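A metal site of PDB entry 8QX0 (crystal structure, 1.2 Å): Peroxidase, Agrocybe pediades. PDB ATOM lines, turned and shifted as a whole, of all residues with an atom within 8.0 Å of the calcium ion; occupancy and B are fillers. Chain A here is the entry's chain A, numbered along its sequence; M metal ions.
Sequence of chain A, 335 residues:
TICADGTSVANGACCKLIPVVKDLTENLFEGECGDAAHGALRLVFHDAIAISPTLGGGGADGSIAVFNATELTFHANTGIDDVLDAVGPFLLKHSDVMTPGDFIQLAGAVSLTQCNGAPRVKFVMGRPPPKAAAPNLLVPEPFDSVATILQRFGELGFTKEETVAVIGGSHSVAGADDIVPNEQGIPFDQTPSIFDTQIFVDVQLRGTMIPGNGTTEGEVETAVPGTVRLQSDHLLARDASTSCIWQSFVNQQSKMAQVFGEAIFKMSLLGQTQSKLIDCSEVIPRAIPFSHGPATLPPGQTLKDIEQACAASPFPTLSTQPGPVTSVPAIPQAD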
ATOM      1  N   ASN A 116     -14.186   1.552 -17.297  1.00  0.00           N
ATOM      2  CA  ASN A 116     -14.749   0.411 -17.981  1.00  0.00           C
ATOM      3  C   ASN A 116     -14.148  -0.865 -17.413  1.00  0.00           C
ATOM      4  O   ASN A 116     -12.922  -1.052 -17.413  1.00  0.00           O
ATOM      5  CB  ASN A 116     -14.410   0.537 -19.466  1.00  0.00           C
ATOM      6  CG  ASN A 116     -15.112  -0.505 -20.302  1.00  0.00           C
ATOM      7  OD1 ASN A 116     -14.710  -1.662 -20.326  1.00  0.00           O
ATOM      8  ND2 ASN A 116     -16.164  -0.083 -21.008  1.00  0.00           N
ATOM      9  N   GLY A 168      -1.465  -5.064  -9.482  1.00  0.00           N
ATOM     10  CA  GLY A 168      -1.523  -5.128 -10.928  1.00  0.00           C
ATOM     11  C   GLY A 168      -2.810  -4.534 -11.476  1.00  0.00           C
ATOM     12  O   GLY A 168      -2.751  -3.715 -12.427  1.00  0.00           O
ATOM     13  N   GLY A 169      -3.979  -4.818 -10.859  1.00  0.00           N
ATOM     14  CA  GLY A 169      -5.226  -4.273 -11.311  1.00  0.00           C
ATOM     15  C   GLY A 169      -5.231  -2.731 -11.240  1.00  0.00           C
ATOM     16  O   GLY A 169      -5.672  -2.039 -12.177  1.00  0.00           O
ATOM     17  N   SER A 170      -4.726  -2.160 -10.124  1.00  0.00           N
ATOM     18  CA  SER A 170      -4.655  -0.720 -10.010  1.00  0.00           C
ATOM     19  C   SER A 170      -3.838  -0.134 -11.172  1.00  0.00           C
ATOM     20  O   SER A 170      -4.139   0.952 -11.680  1.00  0.00           O
ATOM     21  CB  SER A 170      -4.151  -0.264  -8.708  1.00  0.00           C
ATOM     22  OG  SER A 170      -5.094  -0.555  -7.669  1.00  0.00           O
ATOM     23  N   HIS A 171      -2.717  -0.779 -11.485  1.00  0.00           N
ATOM     24  CA  HIS A 171      -1.793  -0.300 -12.484  1.00  0.00           C
ATOM     25  C   HIS A 171      -2.329  -0.454 -13.887  1.00  0.00           C
ATOM     26  O   HIS A 171      -1.752   0.124 -14.798  1.00  0.00           O
ATOM     27  CB  HIS A 171      -0.383  -0.832 -12.217  1.00  0.00           C
ATOM     28  CG  HIS A 171       0.272  -0.258 -10.997  1.00  0.00           C
ATOM     29  ND1 HIS A 171       1.507  -0.646 -10.524  1.00  0.00           N
ATOM     30  CD2 HIS A 171      -0.176   0.663 -10.034  1.00  0.00           C
ATOM     31  CE1 HIS A 171       1.732  -0.008  -9.379  1.00  0.00           C
ATOM     32  NE2 HIS A 171       0.768   0.808  -9.085  1.00  0.00           N
ATOM     33  N   SER A 172      -3.471  -1.138 -14.032  1.00  0.00           N
ATOM     34  CA  SER A 172      -4.232  -1.113 -15.274  1.00  0.00           C
ATOM     35  C   SER A 172      -4.833   0.248 -15.588  1.00  0.00           C
ATOM     36  O   SER A 172      -5.174   0.521 -16.738  1.00  0.00           O
ATOM     37  CB  SER A 172      -5.277  -2.208 -15.277  1.00  0.00           C
ATOM     38  OG  SER A 172      -5.811  -2.312 -16.593  1.00  0.00           O
ATOM     39  N   VAL A 173      -5.006   1.086 -14.573  1.00  0.00           N
ATOM     40  CA  VAL A 173      -5.713   2.340 -14.723  1.00  0.00           C
ATOM     41  C   VAL A 173      -4.894   3.434 -14.005  1.00  0.00           C
ATOM     42  O   VAL A 173      -5.292   3.995 -12.963  1.00  0.00           O
ATOM     43  CB  VAL A 173      -7.161   2.236 -14.202  1.00  0.00           C
ATOM     44  CG1 VAL A 173      -8.039   1.465 -15.185  1.00  0.00           C
ATOM     45  CG2 VAL A 173      -7.254   1.656 -12.808  1.00  0.00           C
ATOM     46  N   ALA A 174      -3.696   3.719 -14.555  1.00  0.00           N
ATOM     47  CA  ALA A 174      -2.701   4.447 -13.774  1.00  0.00           C
ATOM     48  C   ALA A 174      -1.550   4.903 -14.628  1.00  0.00           C
ATOM     49  O   ALA A 174      -1.150   4.255 -15.597  1.00  0.00           O
ATOM     50  CB  ALA A 174      -2.120   3.564 -12.687  1.00  0.00           C
ATOM     51  N   PRO A 187       1.628   6.134 -18.762  1.00  0.00           N
ATOM     52  CA  PRO A 187       0.882   4.965 -18.266  1.00  0.00           C
ATOM     53  C   PRO A 187       1.732   3.738 -18.016  1.00  0.00           C
ATOM     54  O   PRO A 187       2.760   3.510 -18.649  1.00  0.00           O
ATOM     55  CB  PRO A 187      -0.182   4.712 -19.335  1.00  0.00           C
ATOM     56  CG  PRO A 187      -0.200   6.041 -20.146  1.00  0.00           C
ATOM     57  CD  PRO A 187       1.189   6.575 -20.115  1.00  0.00           C
ATOM     58  N   PHE A 188       1.264   2.892 -17.119  1.00  0.00           N
ATOM     59  CA  PHE A 188       1.865   1.599 -16.904  1.00  0.00           C
ATOM     60  C   PHE A 188       1.400   0.545 -17.918  1.00  0.00           C
ATOM     61  O   PHE A 188       2.152  -0.382 -18.241  1.00  0.00           O
ATOM     62  CB  PHE A 188       1.577   1.043 -15.514  1.00  0.00           C
ATOM     63  CG  PHE A 188       2.096   1.962 -14.411  1.00  0.00           C
ATOM     64  CD1 PHE A 188       3.456   2.250 -14.278  1.00  0.00           C
ATOM     65  CD2 PHE A 188       1.243   2.418 -13.406  1.00  0.00           C
ATOM     66  CE1 PHE A 188       3.936   3.086 -13.266  1.00  0.00           C
ATOM     67  CE2 PHE A 188       1.719   3.204 -12.381  1.00  0.00           C
ATOM     68  CZ  PHE A 188       3.064   3.558 -12.303  1.00  0.00           C
ATOM     69  N   ASP A 189       0.180   0.687 -18.479  1.00  0.00           N
ATOM     70  CA  ASP A 189      -0.262  -0.208 -19.528  1.00  0.00           C
ATOM     71  C   ASP A 189      -0.793   0.588 -20.718  1.00  0.00           C
ATOM     72  O   ASP A 189      -0.837   1.814 -20.701  1.00  0.00           O
ATOM     73  CB  ASP A 189      -1.223  -1.262 -19.020  1.00  0.00           C
ATOM     74  CG  ASP A 189      -2.720  -1.045 -18.955  1.00  0.00           C
ATOM     75  OD1 ASP A 189      -3.178   0.101 -19.192  1.00  0.00           O
ATOM     76  OD2 ASP A 189      -3.412  -2.022 -18.558  1.00  0.00           O
ATOM     77  N   GLN A 190      -1.178  -0.160 -21.765  1.00  0.00           N
ATOM     78  CA  GLN A 190      -1.607   0.482 -23.006  1.00  0.00           C
ATOM     79  C   GLN A 190      -2.967   1.154 -22.934  1.00  0.00           C
ATOM     80  O   GLN A 190      -3.272   1.998 -23.804  1.00  0.00           O
ATOM     81  CB  GLN A 190      -1.732  -0.586 -24.095  1.00  0.00           C
ATOM     82  CG  GLN A 190      -0.435  -1.248 -24.469  1.00  0.00           C
ATOM     83  CD  GLN A 190      -0.710  -2.607 -25.059  1.00  0.00           C
ATOM     84  OE1 GLN A 190      -0.775  -3.640 -24.386  1.00  0.00           O
ATOM     85  NE2 GLN A 190      -1.054  -2.579 -26.344  1.00  0.00           N
ATOM     86  N   THR A 191      -3.698   0.940 -21.835  1.00  0.00           N
ATOM     87  CA  THR A 191      -5.092   1.356 -21.733  1.00  0.00           C
ATOM     88  C   THR A 191      -5.348   1.904 -20.309  1.00  0.00           C
ATOM     89  O   THR A 191      -6.107   1.309 -19.512  1.00  0.00           O
ATOM     90  CB  THR A 191      -5.980   0.126 -21.968  1.00  0.00           C
ATOM     91  OG1 THR A 191      -5.619  -0.936 -21.090  1.00  0.00           O
ATOM     92  CG2 THR A 191      -5.941  -0.302 -23.433  1.00  0.00           C
ATOM     93  N   PRO A 192      -4.792   3.085 -19.913  1.00  0.00           N
ATOM     94  CA  PRO A 192      -4.973   3.564 -18.550  1.00  0.00           C
ATOM     95  C   PRO A 192      -6.399   3.990 -18.221  1.00  0.00           C
ATOM     96  O   PRO A 192      -6.696   4.232 -17.057  1.00  0.00           O
ATOM     97  CB  PRO A 192      -3.995   4.713 -18.425  1.00  0.00           C
ATOM     98  CG  PRO A 192      -3.890   5.238 -19.871  1.00  0.00           C
ATOM     99  CD  PRO A 192      -3.873   3.936 -20.674  1.00  0.00           C
ATOM    100  N   SER A 193      -7.323   4.077 -19.220  1.00  0.00           N
ATOM    101  CA  SER A 193      -8.728   4.362 -19.055  1.00  0.00           C
ATOM    102  C   SER A 193      -9.584   3.089 -18.987  1.00  0.00           C
ATOM    103  O   SER A 193     -10.806   3.217 -18.892  1.00  0.00           O
ATOM    104  CB  SER A 193      -9.167   5.420 -20.097  1.00  0.00           C
ATOM    105  OG  SER A 193      -9.498   4.557 -21.166  1.00  0.00           O
ATOM    106  N   ILE A 194      -9.004   1.908 -19.055  1.00  0.00           N
ATOM    107  CA  ILE A 194      -9.764   0.667 -19.154  1.00  0.00           C
ATOM    108  C   ILE A 194      -9.206  -0.314 -18.152  1.00  0.00           C
ATOM    109  O   ILE A 194      -7.986  -0.620 -18.116  1.00  0.00           O
ATOM    110  CB  ILE A 194      -9.696   0.018 -20.549  1.00  0.00           C
ATOM    111  CG1 ILE A 194     -10.152   0.988 -21.604  1.00  0.00           C
ATOM    112  CG2 ILE A 194     -10.514  -1.281 -20.548  1.00  0.00           C
ATOM    113  CD1 ILE A 194      -9.946   0.539 -23.018  1.00  0.00           C
ATOM    114  N   PHE A 195     -10.063  -0.847 -17.276  1.00  0.00           N
ATOM    115  CA  PHE A 195      -9.715  -1.812 -16.256  1.00  0.00           C
ATOM    116  C   PHE A 195      -9.657  -3.196 -16.894  1.00  0.00           C
ATOM    117  O   PHE A 195     -10.552  -4.011 -16.665  1.00  0.00           O
ATOM    118  CB  PHE A 195     -10.680  -1.716 -15.083  1.00  0.00           C
ATOM    119  CG  PHE A 195     -10.208  -2.377 -13.821  1.00  0.00           C
ATOM    120  CD1 PHE A 195      -9.400  -1.646 -12.966  1.00  0.00           C
ATOM    121  CD2 PHE A 195     -10.545  -3.682 -13.486  1.00  0.00           C
ATOM    122  CE1 PHE A 195      -8.914  -2.218 -11.819  1.00  0.00           C
ATOM    123  CE2 PHE A 195     -10.077  -4.229 -12.286  1.00  0.00           C
ATOM    124  CZ  PHE A 195      -9.254  -3.496 -11.474  1.00  0.00           C
ATOM    125  N   ASP A 196      -8.611  -3.441 -17.659  1.00  0.00           N
ATOM    126  CA  ASP A 196      -8.411  -4.692 -18.379  1.00  0.00           C
ATOM    127  C   ASP A 196      -7.158  -5.371 -17.854  1.00  0.00           C
ATOM    128  O   ASP A 196      -6.571  -4.933 -16.849  1.00  0.00           O
ATOM    129  CB  ASP A 196      -8.291  -4.413 -19.874  1.00  0.00           C
ATOM    130  CG  ASP A 196      -7.285  -3.369 -20.265  1.00  0.00           C
ATOM    131  OD1 ASP A 196      -6.410  -3.014 -19.363  1.00  0.00           O
ATOM    132  OD2 ASP A 196      -7.260  -2.913 -21.405  1.00  0.00           O
ATOM    133  N   THR A 197      -6.744  -6.481 -18.522  1.00  0.00           N
ATOM    134  CA  THR A 197      -5.567  -7.203 -18.078  1.00  0.00           C
ATOM    135  C   THR A 197      -4.344  -6.914 -18.955  1.00  0.00           C
ATOM    136  O   THR A 197      -3.330  -7.610 -18.837  1.00  0.00           O
ATOM    137  CB  THR A 197      -5.885  -8.713 -18.000  1.00  0.00           C
ATOM    138  OG1 THR A 197      -6.007  -9.278 -19.315  1.00  0.00           O
ATOM    139  CG2 THR A 197      -7.106  -9.029 -17.170  1.00  0.00           C
ATOM    140  N   GLN A 198      -4.337  -5.810 -19.710  1.00  0.00           N
ATOM    141  CA  GLN A 198      -3.171  -5.405 -20.504  1.00  0.00           C
ATOM    142  C   GLN A 198      -1.922  -5.221 -19.638  1.00  0.00           C
ATOM    143  O   GLN A 198      -0.837  -5.573 -20.049  1.00  0.00           O
ATOM    144  CB  GLN A 198      -3.431  -4.194 -21.393  1.00  0.00           C
ATOM    145  CG  GLN A 198      -4.396  -4.480 -22.555  1.00  0.00           C
ATOM    146  CD  GLN A 198      -3.996  -5.671 -23.413  1.00  0.00           C
ATOM    147  OE1 GLN A 198      -4.676  -6.694 -23.471  1.00  0.00           O
ATOM    148  NE2 GLN A 198      -2.818  -5.627 -23.972  1.00  0.00           N
ATOM    149  N   ILE A 199      -2.106  -4.662 -18.406  1.00  0.00           N
ATOM    150  CA  ILE A 199      -0.955  -4.472 -17.495  1.00  0.00           C
ATOM    151  C   ILE A 199      -0.206  -5.795 -17.373  1.00  0.00           C
ATOM    152  O   ILE A 199       1.041  -5.829 -17.292  1.00  0.00           O
ATOM    153  CB  ILE A 199      -1.428  -3.887 -16.131  1.00  0.00           C
ATOM    154  CG1 ILE A 199      -0.236  -3.677 -15.184  1.00  0.00           C
ATOM    155  CG2 ILE A 199      -2.514  -4.731 -15.463  1.00  0.00           C
ATOM    156  CD1 ILE A 199       0.725  -2.609 -15.650  1.00  0.00           C
ATOM    157  N   PHE A 200      -0.931  -6.905 -17.109  1.00  0.00           N
ATOM    158  CA  PHE A 200      -0.299  -8.206 -16.849  1.00  0.00           C
ATOM    159  C   PHE A 200       0.528  -8.655 -18.059  1.00  0.00           C
ATOM    160  O   PHE A 200       1.627  -9.183 -17.883  1.00  0.00           O
ATOM    161  CB  PHE A 200      -1.323  -9.268 -16.433  1.00  0.00           C
ATOM    162  CG  PHE A 200      -2.027  -8.930 -15.123  1.00  0.00           C
ATOM    163  CD1 PHE A 200      -1.358  -9.182 -13.923  1.00  0.00           C
ATOM    164  CD2 PHE A 200      -3.256  -8.270 -15.112  1.00  0.00           C
ATOM    165  CE1 PHE A 200      -1.945  -8.810 -12.719  1.00  0.00           C
ATOM    166  CE2 PHE A 200      -3.786  -7.876 -13.878  1.00  0.00           C
ATOM    167  CZ  PHE A 200      -3.164  -8.172 -12.729  1.00  0.00           C
ATOM    168  N   ASP A 202       1.684  -6.568 -20.496  1.00  0.00           N
ATOM    169  CA  ASP A 202       2.665  -5.548 -20.851  1.00  0.00           C
ATOM    170  C   ASP A 202       3.937  -5.783 -20.014  1.00  0.00           C
ATOM    171  O   ASP A 202       5.064  -5.634 -20.481  1.00  0.00           O
ATOM    172  CB  ASP A 202       2.125  -4.159 -20.584  1.00  0.00           C
ATOM    173  CG  ASP A 202       1.070  -3.778 -21.583  1.00  0.00           C
ATOM    174  OD1 ASP A 202       1.043  -4.417 -22.685  1.00  0.00           O
ATOM    175  OD2 ASP A 202       0.362  -2.783 -21.373  1.00  0.00           O
ATOM    176  N   MET A 256      -9.921 -11.262 -12.338  1.00  0.00           N
ATOM    177  CA  MET A 256      -9.093 -10.198 -11.798  1.00  0.00           C
ATOM    178  C   MET A 256      -9.946  -9.125 -11.118  1.00  0.00           C
ATOM    179  O   MET A 256      -9.637  -8.744  -9.981  1.00  0.00           O
ATOM    180  CB  MET A 256      -8.232  -9.700 -12.940  1.00  0.00           C
ATOM    181  CG  MET A 256      -7.153  -8.742 -12.448  1.00  0.00           C
ATOM    182  SD  MET A 256      -7.742  -7.049 -12.256  1.00  0.00           S
ATOM    183  CE  MET A 256      -7.611  -6.635 -14.004  1.00  0.00           C
ATOM    184  N   PHE A 290     -17.372  -4.449 -18.507  1.00  0.00           N
ATOM    185  CA  PHE A 290     -16.222  -4.593 -19.357  1.00  0.00           C
ATOM    186  C   PHE A 290     -16.696  -4.810 -20.781  1.00  0.00           C
ATOM    187  O   PHE A 290     -17.486  -5.748 -21.005  1.00  0.00           O
ATOM    188  CB  PHE A 290     -15.328  -5.734 -18.904  1.00  0.00           C
ATOM    189  CG  PHE A 290     -14.046  -5.832 -19.708  1.00  0.00           C
ATOM    190  CD1 PHE A 290     -13.164  -4.769 -19.776  1.00  0.00           C
ATOM    191  CD2 PHE A 290     -13.711  -7.008 -20.359  1.00  0.00           C
ATOM    192  CE1 PHE A 290     -12.009  -4.846 -20.521  1.00  0.00           C
ATOM    193  CE2 PHE A 290     -12.534  -7.091 -21.064  1.00  0.00           C
ATOM    194  CZ  PHE A 290     -11.703  -6.020 -21.163  1.00  0.00           C
HETATM  195 CA    CA M   1      -5.591  -0.879 -18.632  1.00  0.00          CA
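Of the 25 residues printed, 5 come within 4 Å of the calcium ion.
The nearest printed residue that does not touch the calcium ion is Pro 192 (4.2 Å).
OD2 of Asp 189 lies close to N of Ile 199 (2.9 Å).
The backbone NH of Gln 198 lies close to the side-chain carboxylate of Asp 196 (3.5 Å).
The calcium ion is bound by the backbone carbonyl oxygen (O) of Ser 172 (2.4 Å), the side-chain carboxylate (OD1) of Asp 196 (2.4 Å), the backbone carbonyl oxygen (O) of Thr 191 (2.4 Å), the side-chain hydroxyl (OG1) of Thr 191 (2.5 Å), the side-chain carboxylate (OD2) of Asp 189 (2.5 Å), the backbone carbonyl oxygen (O) of Ile 194 (2.5 Å), the side-chain hydroxyl (OG) of Ser 172 (2.5 Å) and the side-chain carboxylate (OD1) of Asp 189 (2.7 Å).
The calcium ion has eight donor atoms within binding distance.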
